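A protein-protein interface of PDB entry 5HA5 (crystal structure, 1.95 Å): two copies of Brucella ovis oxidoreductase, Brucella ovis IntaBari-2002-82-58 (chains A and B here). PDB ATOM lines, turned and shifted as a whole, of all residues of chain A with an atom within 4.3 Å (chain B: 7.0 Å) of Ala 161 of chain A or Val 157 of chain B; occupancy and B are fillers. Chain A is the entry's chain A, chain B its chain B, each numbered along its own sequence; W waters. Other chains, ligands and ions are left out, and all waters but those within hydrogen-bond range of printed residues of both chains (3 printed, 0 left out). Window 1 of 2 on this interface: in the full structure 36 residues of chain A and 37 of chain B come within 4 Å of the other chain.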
ATOM      1  N   LEU A 116      19.415  -4.281 -15.513  1.00  0.00           N
ATOM      2  CA  LEU A 116      20.133  -5.070 -16.499  1.00  0.00           C
ATOM      3  C   LEU A 116      19.604  -6.492 -16.584  1.00  0.00           C
ATOM      4  O   LEU A 116      19.246  -6.955 -17.667  1.00  0.00           O
ATOM      5  CB  LEU A 116      21.635  -5.089 -16.182  1.00  0.00           C
ATOM      6  CG  LEU A 116      22.445  -6.070 -17.036  1.00  0.00           C
ATOM      7  CD1 LEU A 116      22.341  -5.723 -18.516  1.00  0.00           C
ATOM      8  CD2 LEU A 116      23.914  -6.113 -16.584  1.00  0.00           C
ATOM      9  N   VAL A 157      26.514   1.520 -14.264  1.00  0.00           N
ATOM     10  CA  VAL A 157      26.941   0.286 -14.919  1.00  0.00           C
ATOM     11  C   VAL A 157      25.761  -0.404 -15.585  1.00  0.00           C
ATOM     12  O   VAL A 157      25.882  -0.944 -16.691  1.00  0.00           O
ATOM     13  CB  VAL A 157      27.647  -0.626 -13.898  1.00  0.00           C
ATOM     14  CG1 VAL A 157      27.904  -2.016 -14.482  1.00  0.00           C
ATOM     15  CG2 VAL A 157      28.944   0.032 -13.419  1.00  0.00           C
ATOM     16  N   SER A 158      24.599  -0.402 -14.938  1.00  0.00           N
ATOM     17  CA  SER A 158      23.449  -1.040 -15.569  1.00  0.00           C
ATOM     18  C   SER A 158      23.102  -0.359 -16.884  1.00  0.00           C
ATOM     19  O   SER A 158      22.725  -1.026 -17.850  1.00  0.00           O
ATOM     20  CB  SER A 158      22.239  -1.049 -14.627  1.00  0.00           C
ATOM     21  OG  SER A 158      21.600   0.221 -14.523  1.00  0.00           O
ATOM     22  N   LYS A 159      23.252   0.962 -16.958  1.00  0.00           N
ATOM     23  CA  LYS A 159      22.856   1.651 -18.184  1.00  0.00           C
ATOM     24  C   LYS A 159      23.925   1.556 -19.266  1.00  0.00           C
ATOM     25  O   LYS A 159      23.593   1.487 -20.456  1.00  0.00           O
ATOM     26  CB  LYS A 159      22.518   3.113 -17.867  1.00  0.00           C
ATOM     27  CG  LYS A 159      21.324   3.252 -16.910  1.00  0.00           C
ATOM     28  CD  LYS A 159      20.039   2.703 -17.561  1.00  0.00           C
ATOM     29  CE  LYS A 159      18.839   2.702 -16.608  1.00  0.00           C
ATOM     30  NZ  LYS A 159      17.570   2.282 -17.305  1.00  0.00           N
ATOM     31  N   GLY A 160      25.208   1.545 -18.894  1.00  0.00           N
ATOM     32  CA  GLY A 160      26.232   1.218 -19.876  1.00  0.00           C
ATOM     33  C   GLY A 160      26.078  -0.199 -20.406  1.00  0.00           C
ATOM     34  O   GLY A 160      26.275  -0.457 -21.600  1.00  0.00           O
ATOM     35  N   ALA A 161      25.702  -1.129 -19.530  1.00  0.00           N
ATOM     36  CA  ALA A 161      25.391  -2.494 -19.962  1.00  0.00           C
ATOM     37  C   ALA A 161      24.221  -2.515 -20.936  1.00  0.00           C
ATOM     38  O   ALA A 161      24.237  -3.265 -21.924  1.00  0.00           O
ATOM     39  CB  ALA A 161      25.073  -3.373 -18.749  1.00  0.00           C
ATOM     40  N   ILE A 162      23.191  -1.704 -20.672  1.00  0.00           N
ATOM     41  CA  ILE A 162      22.032  -1.634 -21.565  1.00  0.00           C
ATOM     42  C   ILE A 162      22.443  -1.102 -22.927  1.00  0.00           C
ATOM     43  O   ILE A 162      21.919  -1.524 -23.968  1.00  0.00           O
ATOM     44  CB  ILE A 162      20.934  -0.758 -20.930  1.00  0.00           C
ATOM     45  CG1 ILE A 162      20.245  -1.504 -19.781  1.00  0.00           C
ATOM     46  CG2 ILE A 162      19.937  -0.263 -21.980  1.00  0.00           C
ATOM     47  CD1 ILE A 162      19.520  -2.735 -20.191  1.00  0.00           C
ATOM     48  N   ARG A 163      23.355  -0.133 -22.942  1.00  0.00           N
ATOM     49  CA  ARG A 163      23.878   0.368 -24.208  1.00  0.00           C
ATOM     50  C   ARG A 163      24.517  -0.754 -25.023  1.00  0.00           C
ATOM     51  O   ARG A 163      24.259  -0.896 -26.227  1.00  0.00           O
ATOM     52  CB  ARG A 163      24.886   1.479 -23.922  1.00  0.00           C
ATOM     53  CG  ARG A 163      25.589   2.086 -25.131  1.00  0.00           C
ATOM     54  CD  ARG A 163      26.581   3.108 -24.574  1.00  0.00           C
ATOM     55  NE  ARG A 163      27.487   3.677 -25.568  1.00  0.00           N
ATOM     56  CZ  ARG A 163      28.569   4.390 -25.258  1.00  0.00           C
ATOM     57  NH1 ARG A 163      28.879   4.609 -23.985  1.00  0.00           N
ATOM     58  NH2 ARG A 163      29.346   4.878 -26.219  1.00  0.00           N
ATOM     59  N   SER A 164      25.364  -1.564 -24.382  1.00  0.00           N
ATOM     60  CA  SER A 164      25.969  -2.701 -25.076  1.00  0.00           C
ATOM     61  C   SER A 164      24.936  -3.776 -25.417  1.00  0.00           C
ATOM     62  O   SER A 164      25.015  -4.413 -26.479  1.00  0.00           O
ATOM     63  CB  SER A 164      27.081  -3.286 -24.214  1.00  0.00           C
ATOM     64  OG  SER A 164      28.175  -2.386 -24.136  1.00  0.00           O
ATOM     65  N   LEU A 165      23.986  -4.023 -24.519  1.00  0.00           N
ATOM     66  CA  LEU A 165      22.917  -4.973 -24.821  1.00  0.00           C
ATOM     67  C   LEU A 165      22.170  -4.579 -26.091  1.00  0.00           C
ATOM     68  O   LEU A 165      21.792  -5.443 -26.897  1.00  0.00           O
ATOM     69  CB  LEU A 165      21.947  -5.057 -23.644  1.00  0.00           C
ATOM     70  CG  LEU A 165      20.753  -6.008 -23.826  1.00  0.00           C
ATOM     71  CD1 LEU A 165      21.208  -7.467 -23.973  1.00  0.00           C
ATOM     72  CD2 LEU A 165      19.730  -5.854 -22.676  1.00  0.00           C
ATOM     73  N   PHE B  99      21.878 -14.606 -29.286  1.00  0.00           N
ATOM     74  CA  PHE B  99      20.886 -14.118 -28.332  1.00  0.00           C
ATOM     75  C   PHE B  99      19.578 -14.897 -28.412  1.00  0.00           C
ATOM     76  O   PHE B  99      18.914 -15.079 -27.390  1.00  0.00           O
ATOM     77  CB  PHE B  99      20.625 -12.627 -28.554  1.00  0.00           C
ATOM     78  CG  PHE B  99      19.880 -11.973 -27.424  1.00  0.00           C
ATOM     79  CD1 PHE B  99      18.501 -11.808 -27.485  1.00  0.00           C
ATOM     80  CD2 PHE B  99      20.558 -11.557 -26.286  1.00  0.00           C
ATOM     81  CE1 PHE B  99      17.811 -11.207 -26.434  1.00  0.00           C
ATOM     82  CE2 PHE B  99      19.878 -10.958 -25.226  1.00  0.00           C
ATOM     83  CZ  PHE B  99      18.503 -10.790 -25.303  1.00  0.00           C
ATOM     84  N   TRP B 108      25.267 -16.206 -20.626  1.00  0.00           N
ATOM     85  CA  TRP B 108      25.111 -14.886 -20.022  1.00  0.00           C
ATOM     86  C   TRP B 108      25.447 -14.900 -18.533  1.00  0.00           C
ATOM     87  O   TRP B 108      26.261 -14.094 -18.056  1.00  0.00           O
ATOM     88  CB  TRP B 108      23.676 -14.407 -20.241  1.00  0.00           C
ATOM     89  CG  TRP B 108      23.314 -13.112 -19.574  1.00  0.00           C
ATOM     90  CD1 TRP B 108      22.910 -12.939 -18.274  1.00  0.00           C
ATOM     91  CD2 TRP B 108      23.279 -11.816 -20.183  1.00  0.00           C
ATOM     92  NE1 TRP B 108      22.643 -11.614 -18.038  1.00  0.00           N
ATOM     93  CE2 TRP B 108      22.841 -10.906 -19.198  1.00  0.00           C
ATOM     94  CE3 TRP B 108      23.556 -11.340 -21.471  1.00  0.00           C
ATOM     95  CZ2 TRP B 108      22.704  -9.546 -19.450  1.00  0.00           C
ATOM     96  CZ3 TRP B 108      23.403  -9.997 -21.728  1.00  0.00           C
ATOM     97  CH2 TRP B 108      22.988  -9.108 -20.722  1.00  0.00           C
ATOM     98  N   ILE B 112      28.711 -12.841 -17.358  1.00  0.00           N
ATOM     99  CA  ILE B 112      28.450 -11.695 -16.485  1.00  0.00           C
ATOM    100  C   ILE B 112      29.033 -11.938 -15.093  1.00  0.00           C
ATOM    101  O   ILE B 112      29.586 -11.025 -14.460  1.00  0.00           O
ATOM    102  CB  ILE B 112      26.937 -11.405 -16.411  1.00  0.00           C
ATOM    103  CG1 ILE B 112      26.403 -10.889 -17.753  1.00  0.00           C
ATOM    104  CG2 ILE B 112      26.644 -10.417 -15.281  1.00  0.00           C
ATOM    105  CD1 ILE B 112      26.880  -9.482 -18.131  1.00  0.00           C
ATOM    106  N   LEU B 116      31.903  -9.168 -14.976  1.00  0.00           N
ATOM    107  CA  LEU B 116      31.362  -7.962 -14.366  1.00  0.00           C
ATOM    108  C   LEU B 116      31.244  -8.104 -12.853  1.00  0.00           C
ATOM    109  O   LEU B 116      31.802  -7.294 -12.106  1.00  0.00           O
ATOM    110  CB  LEU B 116      29.993  -7.605 -14.971  1.00  0.00           C
ATOM    111  CG  LEU B 116      29.267  -6.466 -14.238  1.00  0.00           C
ATOM    112  CD1 LEU B 116      30.115  -5.189 -14.235  1.00  0.00           C
ATOM    113  CD2 LEU B 116      27.879  -6.193 -14.855  1.00  0.00           C
ATOM    114  N   ALA B 144      34.914  -5.125 -27.545  1.00  0.00           N
ATOM    115  CA  ALA B 144      33.499  -5.474 -27.440  1.00  0.00           C
ATOM    116  C   ALA B 144      32.751  -4.640 -26.402  1.00  0.00           C
ATOM    117  O   ALA B 144      31.523  -4.755 -26.316  1.00  0.00           O
ATOM    118  CB  ALA B 144      33.346  -6.961 -27.111  1.00  0.00           C
ATOM    119  N   GLY B 145      33.451  -3.825 -25.603  1.00  0.00           N
ATOM    120  CA  GLY B 145      32.810  -2.816 -24.781  1.00  0.00           C
ATOM    121  C   GLY B 145      32.366  -1.578 -25.537  1.00  0.00           C
ATOM    122  O   GLY B 145      31.726  -0.697 -24.963  1.00  0.00           O
ATOM    123  N   THR B 152      29.718 -13.159 -27.747  1.00  0.00           N
ATOM    124  CA  THR B 152      28.383 -13.473 -27.249  1.00  0.00           C
ATOM    125  C   THR B 152      27.842 -12.312 -26.414  1.00  0.00           C
ATOM    126  O   THR B 152      28.602 -11.505 -25.857  1.00  0.00           O
ATOM    127  CB  THR B 152      28.397 -14.767 -26.421  1.00  0.00           C
ATOM    128  OG1 THR B 152      27.056 -15.251 -26.246  1.00  0.00           O
ATOM    129  CG2 THR B 152      29.032 -14.548 -25.038  1.00  0.00           C
ATOM    130  N   ALA B 153      26.506 -12.244 -26.329  1.00  0.00           N
ATOM    131  CA  ALA B 153      25.839 -11.133 -25.648  1.00  0.00           C
ATOM    132  C   ALA B 153      26.391 -10.905 -24.249  1.00  0.00           C
ATOM    133  O   ALA B 153      26.696  -9.766 -23.870  1.00  0.00           O
ATOM    134  CB  ALA B 153      24.336 -11.382 -25.576  1.00  0.00           C
ATOM    135  N   GLY B 154      26.522 -11.982 -23.467  1.00  0.00           N
ATOM    136  CA  GLY B 154      27.025 -11.845 -22.110  1.00  0.00           C
ATOM    137  C   GLY B 154      28.410 -11.230 -22.062  1.00  0.00           C
ATOM    138  O   GLY B 154      28.715 -10.433 -21.168  1.00  0.00           O
ATOM    139  N   TYR B 155      29.267 -11.586 -23.024  1.00  0.00           N
ATOM    140  CA  TYR B 155      30.603 -10.991 -23.089  1.00  0.00           C
ATOM    141  C   TYR B 155      30.534  -9.513 -23.464  1.00  0.00           C
ATOM    142  O   TYR B 155      31.144  -8.657 -22.800  1.00  0.00           O
ATOM    143  CB  TYR B 155      31.466 -11.758 -24.096  1.00  0.00           C
ATOM    144  CG  TYR B 155      32.932 -11.366 -24.045  1.00  0.00           C
ATOM    145  CD1 TYR B 155      33.810 -12.006 -23.170  1.00  0.00           C
ATOM    146  CD2 TYR B 155      33.431 -10.338 -24.838  1.00  0.00           C
ATOM    147  CE1 TYR B 155      35.140 -11.648 -23.099  1.00  0.00           C
ATOM    148  CE2 TYR B 155      34.770  -9.978 -24.780  1.00  0.00           C
ATOM    149  CZ  TYR B 155      35.613 -10.640 -23.912  1.00  0.00           C
ATOM    150  OH  TYR B 155      36.942 -10.290 -23.845  1.00  0.00           O
ATOM    151  N   VAL B 156      29.824  -9.199 -24.550  1.00  0.00           N
ATOM    152  CA  VAL B 156      29.697  -7.810 -24.991  1.00  0.00           C
ATOM    153  C   VAL B 156      29.179  -6.944 -23.850  1.00  0.00           C
ATOM    154  O   VAL B 156      29.737  -5.885 -23.538  1.00  0.00           O
ATOM    155  CB  VAL B 156      28.767  -7.719 -26.216  1.00  0.00           C
ATOM    156  CG1 VAL B 156      28.552  -6.255 -26.605  1.00  0.00           C
ATOM    157  CG2 VAL B 156      29.320  -8.527 -27.403  1.00  0.00           C
ATOM    158  N   VAL B 157      28.088  -7.381 -23.219  1.00  0.00           N
ATOM    159  CA  VAL B 157      27.492  -6.599 -22.146  1.00  0.00           C
ATOM    160  C   VAL B 157      28.450  -6.483 -20.969  1.00  0.00           C
ATOM    161  O   VAL B 157      28.568  -5.415 -20.359  1.00  0.00           O
ATOM    162  CB  VAL B 157      26.138  -7.201 -21.727  1.00  0.00           C
ATOM    163  CG1 VAL B 157      25.633  -6.519 -20.468  1.00  0.00           C
ATOM    164  CG2 VAL B 157      25.111  -7.019 -22.855  1.00  0.00           C
ATOM    165  N   SER B 158      29.155  -7.568 -20.629  1.00  0.00           N
ATOM    166  CA  SER B 158      30.064  -7.480 -19.485  1.00  0.00           C
ATOM    167  C   SER B 158      31.153  -6.441 -19.724  1.00  0.00           C
ATOM    168  O   SER B 158      31.545  -5.721 -18.794  1.00  0.00           O
ATOM    169  CB  SER B 158      30.672  -8.852 -19.172  1.00  0.00           C
ATOM    170  OG  SER B 158      31.730  -9.192 -20.064  1.00  0.00           O
ATOM    171  N   LYS B 159      31.612  -6.301 -20.967  1.00  0.00           N
ATOM    172  CA  LYS B 159      32.705  -5.375 -21.231  1.00  0.00           C
ATOM    173  C   LYS B 159      32.211  -3.938 -21.353  1.00  0.00           C
ATOM    174  O   LYS B 159      32.910  -3.007 -20.933  1.00  0.00           O
ATOM    175  CB  LYS B 159      33.472  -5.815 -22.486  1.00  0.00           C
ATOM    176  CG  LYS B 159      34.144  -7.196 -22.308  1.00  0.00           C
ATOM    177  CD  LYS B 159      35.083  -7.241 -21.088  1.00  0.00           C
ATOM    178  CE  LYS B 159      36.019  -8.450 -21.128  1.00  0.00           C
ATOM    179  NZ  LYS B 159      36.961  -8.507 -19.932  1.00  0.00           N
ATOM    180  N   GLY B 160      31.016  -3.723 -21.919  1.00  0.00           N
ATOM    181  CA  GLY B 160      30.421  -2.398 -21.845  1.00  0.00           C
ATOM    182  C   GLY B 160      30.148  -1.979 -20.408  1.00  0.00           C
ATOM    183  O   GLY B 160      30.294  -0.804 -20.049  1.00  0.00           O
ATOM    184  N   ALA B 161      29.780  -2.943 -19.563  1.00  0.00           N
ATOM    185  CA  ALA B 161      29.571  -2.641 -18.151  1.00  0.00           C
ATOM    186  C   ALA B 161      30.886  -2.262 -17.476  1.00  0.00           C
ATOM    187  O   ALA B 161      30.916  -1.371 -16.618  1.00  0.00           O
ATOM    188  CB  ALA B 161      28.936  -3.839 -17.451  1.00  0.00           C
ATOM    189  N   ILE B 162      31.975  -2.940 -17.852  1.00  0.00           N
ATOM    190  CA  ILE B 162      33.304  -2.603 -17.343  1.00  0.00           C
ATOM    191  C   ILE B 162      33.697  -1.195 -17.758  1.00  0.00           C
ATOM    192  O   ILE B 162      34.310  -0.451 -16.983  1.00  0.00           O
ATOM    193  CB  ILE B 162      34.329  -3.642 -17.830  1.00  0.00           C
ATOM    194  CG1 ILE B 162      34.184  -4.932 -17.026  1.00  0.00           C
ATOM    195  CG2 ILE B 162      35.749  -3.083 -17.781  1.00  0.00           C
ATOM    196  CD1 ILE B 162      34.547  -4.789 -15.549  1.00  0.00           C
ATOM    197  N   ARG B 163      33.395  -0.821 -19.000  1.00  0.00           N
ATOM    198  CA  ARG B 163      33.650   0.549 -19.432  1.00  0.00           C
ATOM    199  C   ARG B 163      32.966   1.554 -18.509  1.00  0.00           C
ATOM    200  O   ARG B 163      33.582   2.534 -18.067  1.00  0.00           O
ATOM    201  CB  ARG B 163      33.176   0.699 -20.878  1.00  0.00           C
ATOM    202  CG  ARG B 163      33.376   2.024 -21.544  1.00  0.00           C
ATOM    203  CD  ARG B 163      32.844   1.885 -22.986  1.00  0.00           C
ATOM    204  NE  ARG B 163      32.830   3.145 -23.710  1.00  0.00           N
ATOM    205  CZ  ARG B 163      32.102   3.375 -24.799  1.00  0.00           C
ATOM    206  NH1 ARG B 163      31.313   2.423 -25.295  1.00  0.00           N
ATOM    207  NH2 ARG B 163      32.161   4.562 -25.388  1.00  0.00           N
ATOM    208  N   SER B 164      31.687   1.325 -18.196  1.00  0.00           N
ATOM    209  CA  SER B 164      30.977   2.232 -17.294  1.00  0.00           C
ATOM    210  C   SER B 164      31.500   2.130 -15.873  1.00  0.00           C
ATOM    211  O   SER B 164      31.583   3.143 -15.160  1.00  0.00           O
ATOM    212  CB  SER B 164      29.482   1.933 -17.318  1.00  0.00           C
ATOM    213  OG  SER B 164      28.956   2.308 -18.570  1.00  0.00           O
HETATM  214  O   HOH W   1      31.090   6.460 -23.197  1.00  0.00           O
HETATM  215  O   HOH W   2      30.002   2.574 -28.088  1.00  0.00           O
HETATM  216  O   HOH W   3      29.570  -2.742 -26.412  1.00  0.00           O
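Leu 116 of chain A touches Trp 108 of chain B (CD1 to CZ2, 3.95 Å). Leu 116 of chain A touches Val 157 of chain B. CD1 of Leu 116 of chain B touches CG1 of Val 157 of chain A (3.9 Å). CA of Val 157 of chain A touches CB of Ser 164 of chain B (3.9 Å). OG of Ser 164 of chain B touches CA of Gly 160 of chain A, at 3.2 Å. CG1 of Val 157 of chain B touches CB of Ala 161 of chain A (3.6 Å). Ser 164 of chain A touches Val 156 of chain B (CB to O, 3.8 Å). Gly 160 of chain B touches Ser 164 of chain A. CD1 of Leu 165 of chain A touches CE2 of Phe 99 of chain B (3.9 Å). CA of Leu 165 of chain A touches CG2 of Val 157 of chain B, at 3.6 Å.
Printed residues of chain B that touch a printed residue of chain A: Phe 99, Trp 108, Leu 116, Val 156, Val 157, Gly 160, Ala 161, Arg 163 and Ser 164. Hydrophobic or aromatic side chains of chain B within 4 Å of the printed part of chain A: Phe 99, Trp 108, Leu 116, Val 156, Val 157 and Ala 161. Among the printed residues, 13 pairs touch across the chains. Among the printed residues, no Asp or Glu carboxylate lies within 4 Å of a Lys or Arg side-chain nitrogen of the other chain.
Water W3 lies within hydrogen-bond range of OG of Ser 164 of chain A, O of Ala 144 of chain B and O of Gly 145 of chain B. Water W1 bridges NH1 of Arg 163 of chain A (3.0 Å) and NH2 of Arg 163 of chain B (3.1 Å). Water W2 bridges NH2 of Arg 163 of chain A (3.0 Å) and NH1 of Arg 163 of chain B (3.1 Å).
The guanidinium group of Arg 163 of chain B lies close to the guanidinium group of Arg 163 of chain A (3.0 Å).
The backbone carbonyl oxygen (O) of Gly 145 of chain B is in hydrogen-bond range of the guanidinium group (NH1) of Arg 163 of chain B, at 3.2 Å.
Leu 116 of chain A touches Val 157 of chain B, and with the chains exchanged Val 157 of chain A touches Leu 116 of chain B. Val 157 of chain A touches Ala 161 of chain B, and with the chains exchanged Ala 161 of chain A touches Val 157 of chain B. Gly 160 of chain A touches Ser 164 of chain B, and with the chains exchanged Ser 164 of chain A touches Gly 160 of chain B. Arg 163 of chain B touches its own counterpart, Arg 163 of chain A. 9 positions are printed for both chains.
Printed residues of chain B within 4 Å of Gly 160 of chain A: Ser 164. Of chain B, only Val 157 (3.6 Å) comes within 4 Å of Ala 161 of chain A. Of the printed residues of chain B, Arg 163 of chain A touches Arg 163 (3.0 Å). Of the printed residues of chain A, Phe 99 of chain B touches Leu 165 (3.9 Å). Of the printed residues of chain A, Trp 108 of chain B touches Leu 116. Gly 154 of chain B touches none of the printed residues of chain A. Lys 159 of chain B touches none of the printed residues of chain A. Of the printed residues of chain A, Ala 161 of chain B touches Val 157 (3.6 Å). Printed residues of chain A within 4 Å of Arg 163 of chain B: Arg 163 (3.0 Å). The nearest printed residue of chain A that does not touch Val 157 of chain B is Ile 162 of chain A (5.4 Å). The nearest printed residue of chain B that does not touch Leu 165 of chain A is Trp 108 of chain B (4.03 Å).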
